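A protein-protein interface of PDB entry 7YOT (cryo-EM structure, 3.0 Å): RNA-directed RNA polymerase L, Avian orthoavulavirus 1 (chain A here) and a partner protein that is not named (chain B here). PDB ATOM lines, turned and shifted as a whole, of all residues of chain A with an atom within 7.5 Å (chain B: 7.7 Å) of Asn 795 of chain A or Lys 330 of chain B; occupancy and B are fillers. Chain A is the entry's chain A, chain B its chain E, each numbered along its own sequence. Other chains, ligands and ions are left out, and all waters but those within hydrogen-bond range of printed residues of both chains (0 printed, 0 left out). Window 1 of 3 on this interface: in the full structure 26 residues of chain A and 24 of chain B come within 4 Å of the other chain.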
ATOM      1  N   LYS A 382     -15.408  -7.482  16.310  1.00  0.00           N
ATOM      2  CA  LYS A 382     -16.389  -8.205  15.516  1.00  0.00           C
ATOM      3  C   LYS A 382     -16.714  -7.450  14.239  1.00  0.00           C
ATOM      4  O   LYS A 382     -16.514  -6.241  14.133  1.00  0.00           O
ATOM      5  CB  LYS A 382     -17.692  -8.468  16.268  1.00  0.00           C
ATOM      6  CG  LYS A 382     -17.540  -9.369  17.457  1.00  0.00           C
ATOM      7  CD  LYS A 382     -18.862  -9.800  17.958  1.00  0.00           C
ATOM      8  CE  LYS A 382     -19.365 -10.871  17.103  1.00  0.00           C
ATOM      9  NZ  LYS A 382     -18.488 -12.016  17.354  1.00  0.00           N
ATOM     10  N   THR A 640     -29.926 -26.545  19.890  1.00  0.00           N
ATOM     11  CA  THR A 640     -28.701 -25.827  19.630  1.00  0.00           C
ATOM     12  C   THR A 640     -28.310 -24.999  20.839  1.00  0.00           C
ATOM     13  O   THR A 640     -29.155 -24.522  21.608  1.00  0.00           O
ATOM     14  CB  THR A 640     -28.830 -24.962  18.374  1.00  0.00           C
ATOM     15  OG1 THR A 640     -27.646 -24.187  18.209  1.00  0.00           O
ATOM     16  CG2 THR A 640     -30.011 -24.063  18.439  1.00  0.00           C
ATOM     17  N   ASP A 641     -27.002 -24.893  21.023  1.00  0.00           N
ATOM     18  CA  ASP A 641     -26.413 -24.103  22.089  1.00  0.00           C
ATOM     19  C   ASP A 641     -25.332 -23.249  21.451  1.00  0.00           C
ATOM     20  O   ASP A 641     -24.432 -23.777  20.791  1.00  0.00           O
ATOM     21  CB  ASP A 641     -25.854 -24.999  23.194  1.00  0.00           C
ATOM     22  CG  ASP A 641     -25.700 -24.271  24.499  1.00  0.00           C
ATOM     23  OD1 ASP A 641     -25.977 -23.061  24.534  1.00  0.00           O
ATOM     24  OD2 ASP A 641     -25.327 -24.912  25.500  1.00  0.00           O
ATOM     25  N   LEU A 642     -25.447 -21.938  21.605  1.00  0.00           N
ATOM     26  CA  LEU A 642     -24.589 -21.007  20.893  1.00  0.00           C
ATOM     27  C   LEU A 642     -23.317 -20.760  21.687  1.00  0.00           C
ATOM     28  O   LEU A 642     -23.357 -20.626  22.911  1.00  0.00           O
ATOM     29  CB  LEU A 642     -25.317 -19.688  20.629  1.00  0.00           C
ATOM     30  CG  LEU A 642     -26.340 -19.607  19.484  1.00  0.00           C
ATOM     31  CD1 LEU A 642     -27.674 -20.254  19.801  1.00  0.00           C
ATOM     32  CD2 LEU A 642     -26.566 -18.183  19.060  1.00  0.00           C
ATOM     33  N   GLN A 643     -22.189 -20.714  20.981  1.00  0.00           N
ATOM     34  CA  GLN A 643     -20.889 -20.492  21.607  1.00  0.00           C
ATOM     35  C   GLN A 643     -20.810 -19.079  22.150  1.00  0.00           C
ATOM     36  O   GLN A 643     -20.831 -18.120  21.371  1.00  0.00           O
ATOM     37  CB  GLN A 643     -19.754 -20.719  20.616  1.00  0.00           C
ATOM     38  CG  GLN A 643     -18.401 -20.383  21.205  1.00  0.00           C
ATOM     39  CD  GLN A 643     -17.277 -20.536  20.222  1.00  0.00           C
ATOM     40  OE1 GLN A 643     -17.492 -20.885  19.065  1.00  0.00           O
ATOM     41  NE2 GLN A 643     -16.062 -20.259  20.672  1.00  0.00           N
ATOM     42  N   LYS A 644     -20.720 -18.965  23.481  1.00  0.00           N
ATOM     43  CA  LYS A 644     -20.459 -17.718  24.207  1.00  0.00           C
ATOM     44  C   LYS A 644     -21.478 -16.636  23.856  1.00  0.00           C
ATOM     45  O   LYS A 644     -21.146 -15.588  23.309  1.00  0.00           O
ATOM     46  CB  LYS A 644     -19.026 -17.244  23.964  1.00  0.00           C
ATOM     47  CG  LYS A 644     -17.987 -18.111  24.633  1.00  0.00           C
ATOM     48  CD  LYS A 644     -18.091 -17.992  26.143  1.00  0.00           C
ATOM     49  CE  LYS A 644     -17.084 -18.876  26.847  1.00  0.00           C
ATOM     50  NZ  LYS A 644     -15.691 -18.416  26.631  1.00  0.00           N
ATOM     51  N   TYR A 645     -22.735 -16.924  24.189  1.00  0.00           N
ATOM     52  CA  TYR A 645     -23.868 -16.202  23.619  1.00  0.00           C
ATOM     53  C   TYR A 645     -23.956 -14.774  24.127  1.00  0.00           C
ATOM     54  O   TYR A 645     -24.038 -13.831  23.338  1.00  0.00           O
ATOM     55  CB  TYR A 645     -25.147 -16.954  23.948  1.00  0.00           C
ATOM     56  CG  TYR A 645     -26.419 -16.318  23.469  1.00  0.00           C
ATOM     57  CD1 TYR A 645     -26.797 -16.400  22.142  1.00  0.00           C
ATOM     58  CD2 TYR A 645     -27.255 -15.652  24.353  1.00  0.00           C
ATOM     59  CE1 TYR A 645     -27.962 -15.829  21.702  1.00  0.00           C
ATOM     60  CE2 TYR A 645     -28.422 -15.075  23.923  1.00  0.00           C
ATOM     61  CZ  TYR A 645     -28.771 -15.168  22.596  1.00  0.00           C
ATOM     62  OH  TYR A 645     -29.939 -14.598  22.160  1.00  0.00           O
ATOM     63  N   ASN A 648     -21.209 -12.042  23.091  1.00  0.00           N
ATOM     64  CA  ASN A 648     -20.955 -11.774  21.685  1.00  0.00           C
ATOM     65  C   ASN A 648     -21.961 -10.801  21.100  1.00  0.00           C
ATOM     66  O   ASN A 648     -21.845 -10.445  19.923  1.00  0.00           O
ATOM     67  CB  ASN A 648     -20.963 -13.072  20.875  1.00  0.00           C
ATOM     68  CG  ASN A 648     -19.687 -13.853  21.028  1.00  0.00           C
ATOM     69  OD1 ASN A 648     -18.599 -13.307  20.904  1.00  0.00           O
ATOM     70  ND2 ASN A 648     -19.810 -15.126  21.337  1.00  0.00           N
ATOM     71  N   ILE A 786     -27.222 -21.549  10.776  1.00  0.00           N
ATOM     72  CA  ILE A 786     -25.779 -21.282  10.773  1.00  0.00           C
ATOM     73  C   ILE A 786     -25.481 -19.958  10.089  1.00  0.00           C
ATOM     74  O   ILE A 786     -24.729 -19.123  10.605  1.00  0.00           O
ATOM     75  CB  ILE A 786     -25.023 -22.421  10.061  1.00  0.00           C
ATOM     76  CG1 ILE A 786     -25.106 -23.747  10.800  1.00  0.00           C
ATOM     77  CG2 ILE A 786     -23.564 -22.056   9.834  1.00  0.00           C
ATOM     78  CD1 ILE A 786     -24.397 -23.782  12.046  1.00  0.00           C
ATOM     79  N   ASN A 789     -26.871 -16.761  11.895  1.00  0.00           N
ATOM     80  CA  ASN A 789     -26.194 -16.469  13.151  1.00  0.00           C
ATOM     81  C   ASN A 789     -24.736 -16.083  12.973  1.00  0.00           C
ATOM     82  O   ASN A 789     -24.227 -15.301  13.776  1.00  0.00           O
ATOM     83  CB  ASN A 789     -26.304 -17.657  14.098  1.00  0.00           C
ATOM     84  CG  ASN A 789     -27.574 -17.632  14.888  1.00  0.00           C
ATOM     85  OD1 ASN A 789     -27.914 -16.624  15.492  1.00  0.00           O
ATOM     86  ND2 ASN A 789     -28.307 -18.719  14.861  1.00  0.00           N
ATOM     87  N   HIS A 790     -24.059 -16.592  11.943  1.00  0.00           N
ATOM     88  CA  HIS A 790     -22.683 -16.177  11.691  1.00  0.00           C
ATOM     89  C   HIS A 790     -22.601 -14.717  11.282  1.00  0.00           C
ATOM     90  O   HIS A 790     -21.609 -14.046  11.585  1.00  0.00           O
ATOM     91  CB  HIS A 790     -22.062 -17.056  10.609  1.00  0.00           C
ATOM     92  CG  HIS A 790     -20.663 -16.673  10.243  1.00  0.00           C
ATOM     93  ND1 HIS A 790     -19.576 -16.961  11.038  1.00  0.00           N
ATOM     94  CD2 HIS A 790     -20.178 -16.013   9.168  1.00  0.00           C
ATOM     95  CE1 HIS A 790     -18.480 -16.502  10.462  1.00  0.00           C
ATOM     96  NE2 HIS A 790     -18.818 -15.917   9.331  1.00  0.00           N
ATOM     97  N   LEU A 791     -23.630 -14.199  10.623  1.00  0.00           N
ATOM     98  CA  LEU A 791     -23.559 -12.842  10.109  1.00  0.00           C
ATOM     99  C   LEU A 791     -23.986 -11.793  11.123  1.00  0.00           C
ATOM    100  O   LEU A 791     -23.652 -10.620  10.950  1.00  0.00           O
ATOM    101  CB  LEU A 791     -24.392 -12.725   8.837  1.00  0.00           C
ATOM    102  CG  LEU A 791     -23.807 -13.533   7.680  1.00  0.00           C
ATOM    103  CD1 LEU A 791     -24.656 -13.442   6.458  1.00  0.00           C
ATOM    104  CD2 LEU A 791     -22.423 -13.057   7.360  1.00  0.00           C
ATOM    105  N   ILE A 792     -24.706 -12.176  12.177  1.00  0.00           N
ATOM    106  CA  ILE A 792     -25.011 -11.248  13.259  1.00  0.00           C
ATOM    107  C   ILE A 792     -24.049 -11.510  14.409  1.00  0.00           C
ATOM    108  O   ILE A 792     -24.201 -10.956  15.500  1.00  0.00           O
ATOM    109  CB  ILE A 792     -26.478 -11.345  13.720  1.00  0.00           C
ATOM    110  CG1 ILE A 792     -26.779 -12.689  14.373  1.00  0.00           C
ATOM    111  CG2 ILE A 792     -27.401 -11.133  12.556  1.00  0.00           C
ATOM    112  CD1 ILE A 792     -28.134 -12.732  15.043  1.00  0.00           C
ATOM    113  N   GLY A 793     -23.058 -12.353  14.178  1.00  0.00           N
ATOM    114  CA  GLY A 793     -21.946 -12.492  15.078  1.00  0.00           C
ATOM    115  C   GLY A 793     -22.023 -13.600  16.094  1.00  0.00           C
ATOM    116  O   GLY A 793     -21.445 -13.459  17.173  1.00  0.00           O
ATOM    117  N   HIS A 794     -22.710 -14.692  15.799  1.00  0.00           N
ATOM    118  CA  HIS A 794     -22.847 -15.771  16.757  1.00  0.00           C
ATOM    119  C   HIS A 794     -22.438 -17.088  16.127  1.00  0.00           C
ATOM    120  O   HIS A 794     -22.469 -17.261  14.912  1.00  0.00           O
ATOM    121  CB  HIS A 794     -24.273 -15.867  17.283  1.00  0.00           C
ATOM    122  CG  HIS A 794     -24.657 -14.720  18.154  1.00  0.00           C
ATOM    123  ND1 HIS A 794     -24.193 -14.581  19.439  1.00  0.00           N
ATOM    124  CD2 HIS A 794     -25.444 -13.648  17.919  1.00  0.00           C
ATOM    125  CE1 HIS A 794     -24.682 -13.474  19.962  1.00  0.00           C
ATOM    126  NE2 HIS A 794     -25.448 -12.891  19.062  1.00  0.00           N
ATOM    127  N   ASN A 795     -22.048 -18.023  16.979  1.00  0.00           N
ATOM    128  CA  ASN A 795     -21.591 -19.333  16.543  1.00  0.00           C
ATOM    129  C   ASN A 795     -22.423 -20.385  17.248  1.00  0.00           C
ATOM    130  O   ASN A 795     -22.332 -20.536  18.468  1.00  0.00           O
ATOM    131  CB  ASN A 795     -20.116 -19.533  16.860  1.00  0.00           C
ATOM    132  CG  ASN A 795     -19.523 -20.733  16.182  1.00  0.00           C
ATOM    133  OD1 ASN A 795     -20.171 -21.415  15.394  1.00  0.00           O
ATOM    134  ND2 ASN A 795     -18.279 -21.019  16.511  1.00  0.00           N
ATOM    135  N   LEU A 796     -23.233 -21.101  16.492  1.00  0.00           N
ATOM    136  CA  LEU A 796     -23.708 -22.405  16.910  1.00  0.00           C
ATOM    137  C   LEU A 796     -23.029 -23.418  16.006  1.00  0.00           C
ATOM    138  O   LEU A 796     -22.829 -23.160  14.819  1.00  0.00           O
ATOM    139  CB  LEU A 796     -25.234 -22.490  16.849  1.00  0.00           C
ATOM    140  CG  LEU A 796     -26.097 -22.429  15.595  1.00  0.00           C
ATOM    141  CD1 LEU A 796     -26.432 -23.804  15.101  1.00  0.00           C
ATOM    142  CD2 LEU A 796     -27.350 -21.716  15.946  1.00  0.00           C
ATOM    143  N   LYS A 797     -22.618 -24.537  16.582  1.00  0.00           N
ATOM    144  CA  LYS A 797     -21.676 -25.406  15.900  1.00  0.00           C
ATOM    145  C   LYS A 797     -22.375 -26.282  14.865  1.00  0.00           C
ATOM    146  O   LYS A 797     -23.590 -26.476  14.888  1.00  0.00           O
ATOM    147  CB  LYS A 797     -20.941 -26.267  16.916  1.00  0.00           C
ATOM    148  CG  LYS A 797     -20.187 -25.466  17.962  1.00  0.00           C
ATOM    149  CD  LYS A 797     -18.988 -24.767  17.362  1.00  0.00           C
ATOM    150  CE  LYS A 797     -18.150 -24.113  18.439  1.00  0.00           C
ATOM    151  NZ  LYS A 797     -16.932 -23.476  17.872  1.00  0.00           N
ATOM    152  N   ASP A 798     -21.581 -26.800  13.929  1.00  0.00           N
ATOM    153  CA  ASP A 798     -22.101 -27.769  12.971  1.00  0.00           C
ATOM    154  C   ASP A 798     -22.240 -29.153  13.584  1.00  0.00           C
ATOM    155  O   ASP A 798     -23.056 -29.954  13.118  1.00  0.00           O
ATOM    156  CB  ASP A 798     -21.197 -27.842  11.739  1.00  0.00           C
ATOM    157  CG  ASP A 798     -21.388 -26.669  10.801  1.00  0.00           C
ATOM    158  OD1 ASP A 798     -22.525 -26.172  10.702  1.00  0.00           O
ATOM    159  OD2 ASP A 798     -20.407 -26.246  10.156  1.00  0.00           O
ATOM    160  N   THR A 801     -24.268 -29.071  18.134  1.00  0.00           N
ATOM    161  CA  THR A 801     -25.717 -29.007  18.255  1.00  0.00           C
ATOM    162  C   THR A 801     -26.312 -30.373  17.965  1.00  0.00           C
ATOM    163  O   THR A 801     -25.925 -31.030  16.995  1.00  0.00           O
ATOM    164  CB  THR A 801     -26.288 -27.980  17.289  1.00  0.00           C
ATOM    165  OG1 THR A 801     -26.083 -28.428  15.949  1.00  0.00           O
ATOM    166  CG2 THR A 801     -25.587 -26.668  17.471  1.00  0.00           C
ATOM    167  N   ASP B 287     -14.465 -14.471   5.019  1.00  0.00           N
ATOM    168  CA  ASP B 287     -15.338 -15.422   5.714  1.00  0.00           C
ATOM    169  C   ASP B 287     -15.194 -16.859   5.234  1.00  0.00           C
ATOM    170  O   ASP B 287     -15.482 -17.153   4.068  1.00  0.00           O
ATOM    171  CB  ASP B 287     -16.812 -15.049   5.535  1.00  0.00           C
ATOM    172  CG  ASP B 287     -17.292 -14.046   6.534  1.00  0.00           C
ATOM    173  OD1 ASP B 287     -16.818 -14.098   7.683  1.00  0.00           O
ATOM    174  OD2 ASP B 287     -18.154 -13.219   6.176  1.00  0.00           O
ATOM    175  N   PRO B 288     -14.786 -17.784   6.094  1.00  0.00           N
ATOM    176  CA  PRO B 288     -14.908 -19.203   5.741  1.00  0.00           C
ATOM    177  C   PRO B 288     -16.332 -19.708   5.947  1.00  0.00           C
ATOM    178  O   PRO B 288     -16.664 -20.271   6.994  1.00  0.00           O
ATOM    179  CB  PRO B 288     -13.911 -19.880   6.686  1.00  0.00           C
ATOM    180  CG  PRO B 288     -13.851 -18.972   7.867  1.00  0.00           C
ATOM    181  CD  PRO B 288     -14.041 -17.582   7.347  1.00  0.00           C
ATOM    182  N   GLY B 289     -17.192 -19.497   4.956  1.00  0.00           N
ATOM    183  CA  GLY B 289     -18.577 -19.925   5.058  1.00  0.00           C
ATOM    184  C   GLY B 289     -18.765 -21.432   4.978  1.00  0.00           C
ATOM    185  O   GLY B 289     -19.641 -22.004   5.629  1.00  0.00           O
ATOM    186  N   LEU B 328     -12.054 -13.274   8.898  1.00  0.00           N
ATOM    187  CA  LEU B 328     -12.966 -13.347  10.026  1.00  0.00           C
ATOM    188  C   LEU B 328     -12.984 -14.745  10.625  1.00  0.00           C
ATOM    189  O   LEU B 328     -12.722 -15.740   9.950  1.00  0.00           O
ATOM    190  CB  LEU B 328     -14.385 -12.941   9.631  1.00  0.00           C
ATOM    191  CG  LEU B 328     -14.550 -11.502   9.153  1.00  0.00           C
ATOM    192  CD1 LEU B 328     -15.996 -11.176   8.902  1.00  0.00           C
ATOM    193  CD2 LEU B 328     -13.964 -10.532  10.132  1.00  0.00           C
ATOM    194  N   ASN B 329     -13.330 -14.800  11.907  1.00  0.00           N
ATOM    195  CA  ASN B 329     -13.346 -16.019  12.702  1.00  0.00           C
ATOM    196  C   ASN B 329     -14.629 -16.789  12.400  1.00  0.00           C
ATOM    197  O   ASN B 329     -15.334 -16.522  11.425  1.00  0.00           O
ATOM    198  CB  ASN B 329     -13.246 -15.662  14.183  1.00  0.00           C
ATOM    199  CG  ASN B 329     -12.489 -16.675  14.988  1.00  0.00           C
ATOM    200  OD1 ASN B 329     -12.174 -16.433  16.149  1.00  0.00           O
ATOM    201  ND2 ASN B 329     -12.149 -17.797  14.371  1.00  0.00           N
ATOM    202  N   LYS B 330     -14.951 -17.763  13.241  1.00  0.00           N
ATOM    203  CA  LYS B 330     -16.248 -18.413  13.158  1.00  0.00           C
ATOM    204  C   LYS B 330     -17.310 -17.627  13.917  1.00  0.00           C
ATOM    205  O   LYS B 330     -18.507 -17.867  13.730  1.00  0.00           O
ATOM    206  CB  LYS B 330     -16.111 -19.844  13.680  1.00  0.00           C
ATOM    207  CG  LYS B 330     -17.204 -20.796  13.249  1.00  0.00           C
ATOM    208  CD  LYS B 330     -16.909 -22.212  13.705  1.00  0.00           C
ATOM    209  CE  LYS B 330     -15.782 -22.819  12.898  1.00  0.00           C
ATOM    210  NZ  LYS B 330     -16.181 -23.023  11.480  1.00  0.00           N
ATOM    211  N   LEU B 331     -16.885 -16.674  14.741  1.00  0.00           N
ATOM    212  CA  LEU B 331     -17.736 -15.738  15.458  1.00  0.00           C
ATOM    213  C   LEU B 331     -17.773 -14.363  14.808  1.00  0.00           C
ATOM    214  O   LEU B 331     -18.113 -13.393  15.488  1.00  0.00           O
ATOM    215  CB  LEU B 331     -17.243 -15.600  16.896  1.00  0.00           C
ATOM    216  CG  LEU B 331     -17.484 -16.710  17.904  1.00  0.00           C
ATOM    217  CD1 LEU B 331     -16.489 -16.583  19.001  1.00  0.00           C
ATOM    218  CD2 LEU B 331     -18.840 -16.490  18.475  1.00  0.00           C
ATOM    219  N   SER B 332     -17.409 -14.268  13.522  1.00  0.00           N
ATOM    220  CA  SER B 332     -17.272 -13.007  12.780  1.00  0.00           C
ATOM    221  C   SER B 332     -16.317 -12.042  13.474  1.00  0.00           C
ATOM    222  O   SER B 332     -16.563 -10.838  13.537  1.00  0.00           O
ATOM    223  CB  SER B 332     -18.625 -12.341  12.529  1.00  0.00           C
ATOM    224  OG  SER B 332     -19.410 -13.107  11.643  1.00  0.00           O
ATOM    225  N   GLN B 333     -15.236 -12.567  13.990  1.00  0.00           N
ATOM    226  CA  GLN B 333     -14.215 -11.779  14.654  1.00  0.00           C
ATOM    227  C   GLN B 333     -13.006 -11.632  13.754  1.00  0.00           C
ATOM    228  O   GLN B 333     -12.493 -12.645  13.268  1.00  0.00           O
ATOM    229  CB  GLN B 333     -13.798 -12.440  15.963  1.00  0.00           C
ATOM    230  CG  GLN B 333     -14.874 -12.484  17.025  1.00  0.00           C
ATOM    231  CD  GLN B 333     -14.386 -13.096  18.312  1.00  0.00           C
ATOM    232  OE1 GLN B 333     -13.257 -13.569  18.392  1.00  0.00           O
ATOM    233  NE2 GLN B 333     -15.230 -13.089  19.331  1.00  0.00           N
ATOM    234  N   LEU B 341      -6.969 -19.512  10.775  1.00  0.00           N
ATOM    235  CA  LEU B 341      -8.145 -20.175  10.219  1.00  0.00           C
ATOM    236  C   LEU B 341      -7.849 -21.558   9.652  1.00  0.00           C
ATOM    237  O   LEU B 341      -8.784 -22.223   9.197  1.00  0.00           O
ATOM    238  CB  LEU B 341      -8.775 -19.299   9.135  1.00  0.00           C
ATOM    239  CG  LEU B 341      -9.826 -18.248   9.509  1.00  0.00           C
ATOM    240  CD1 LEU B 341      -9.268 -17.133  10.346  1.00  0.00           C
ATOM    241  CD2 LEU B 341     -10.400 -17.663   8.243  1.00  0.00           C
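Among the printed residues, merely in contact across the chains: Lys 382 of chain A with Ser 332 of chain B (3.3 Å), Lys 382 of chain A with Gln 333 of chain B (3.7 Å), Gln 643 of chain A with Leu 331 of chain B (3.9 Å), Asn 648 of chain A with Leu 331 of chain B (3.3 Å), Asn 648 of chain A with Gln 333 of chain B (3.7 Å), His 790 of chain A with Asn 329 of chain B (3.3 Å), Gly 793 of chain A with Leu 331 of chain B (3.7 Å), Asn 795 of chain A with Lys 330 of chain B (3.3 Å) and Asn 795 of chain A with Leu 331 of chain B (3.7 Å).
Of the printed residues of chain B, Asn 795 of chain A touches Lys 330 (3.3 Å) and Leu 331 (3.7 Å).
Of chain A, only His 790 (3.0 Å) and Asn 795 (3.3 Å) come within 4 Å of Lys 330 of chain B.
Printed residues of chain A within 4 Å of Leu 331 of chain B: Lys 382 (2.3 Å), Gln 643 (3.9 Å), Asn 648 (3.3 Å), Gly 793 (3.7 Å) and Asn 795 (3.7 Å).
Of the printed residues of chain A, Asn 329 of chain B touches His 790 (3.3 Å).
Of the printed residues of chain A, Ser 332 of chain B touches Lys 382 (3.3 Å) and His 790 (2.4 Å).
Ile 792 of chain A touches none of the printed residues of chain B.
O of Lys 644 of chain A sits at hydrogen-bond distance from ND2 of Asn 648 of chain A, at 2.4 Å.
O of Gln 643 of chain A sits at hydrogen-bond distance from ND2 of Asn 648 of chain A (3.2 Å).
The side-chain amino group (NZ) of Lys 382 of chain A is in hydrogen-bond range of the backbone carbonyl oxygen (O) of Gly 793 of chain A, at 3.3 Å.
The backbone carbonyl oxygen of Asn 795 of chain A sits at hydrogen-bond distance from the backbone NH of Gln 643 of chain A, at 2.5 Å.
OE1 of Gln 643 of chain A lies within hydrogen-bond range of NZ of Lys 797 of chain A (2.9 Å).
NZ of Lys 797 of chain A sits close to ND2 of Asn 795 of chain A (3.1 Å).
Printed residues of chain A that touch a printed residue of chain B: Lys 382, Gln 643, Asn 648, His 790, Gly 793 and Asn 795.
Of the 10 printed residues of chain B, 6 touch a printed residue of chain A.
Among the printed residues, no Asp or Glu carboxylate lies within 4 Å of a Lys or Arg side-chain nitrogen of the other chain.
OG of Ser 332 of chain B sits close to O of His 790 of chain A.
The backbone carbonyl oxygen (O) of Lys 330 of chain B is in hydrogen-bond range of a ring nitrogen (ND1) of His 790 of chain A (3.0 Å).
O of Leu 331 of chain B lies close to NZ of Lys 382 of chain A.
The side-chain carboxylate of Asp 287 of chain B sits at hydrogen-bond distance from a ring nitrogen (NE2) of His 790 of chain A (3.2 Å).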
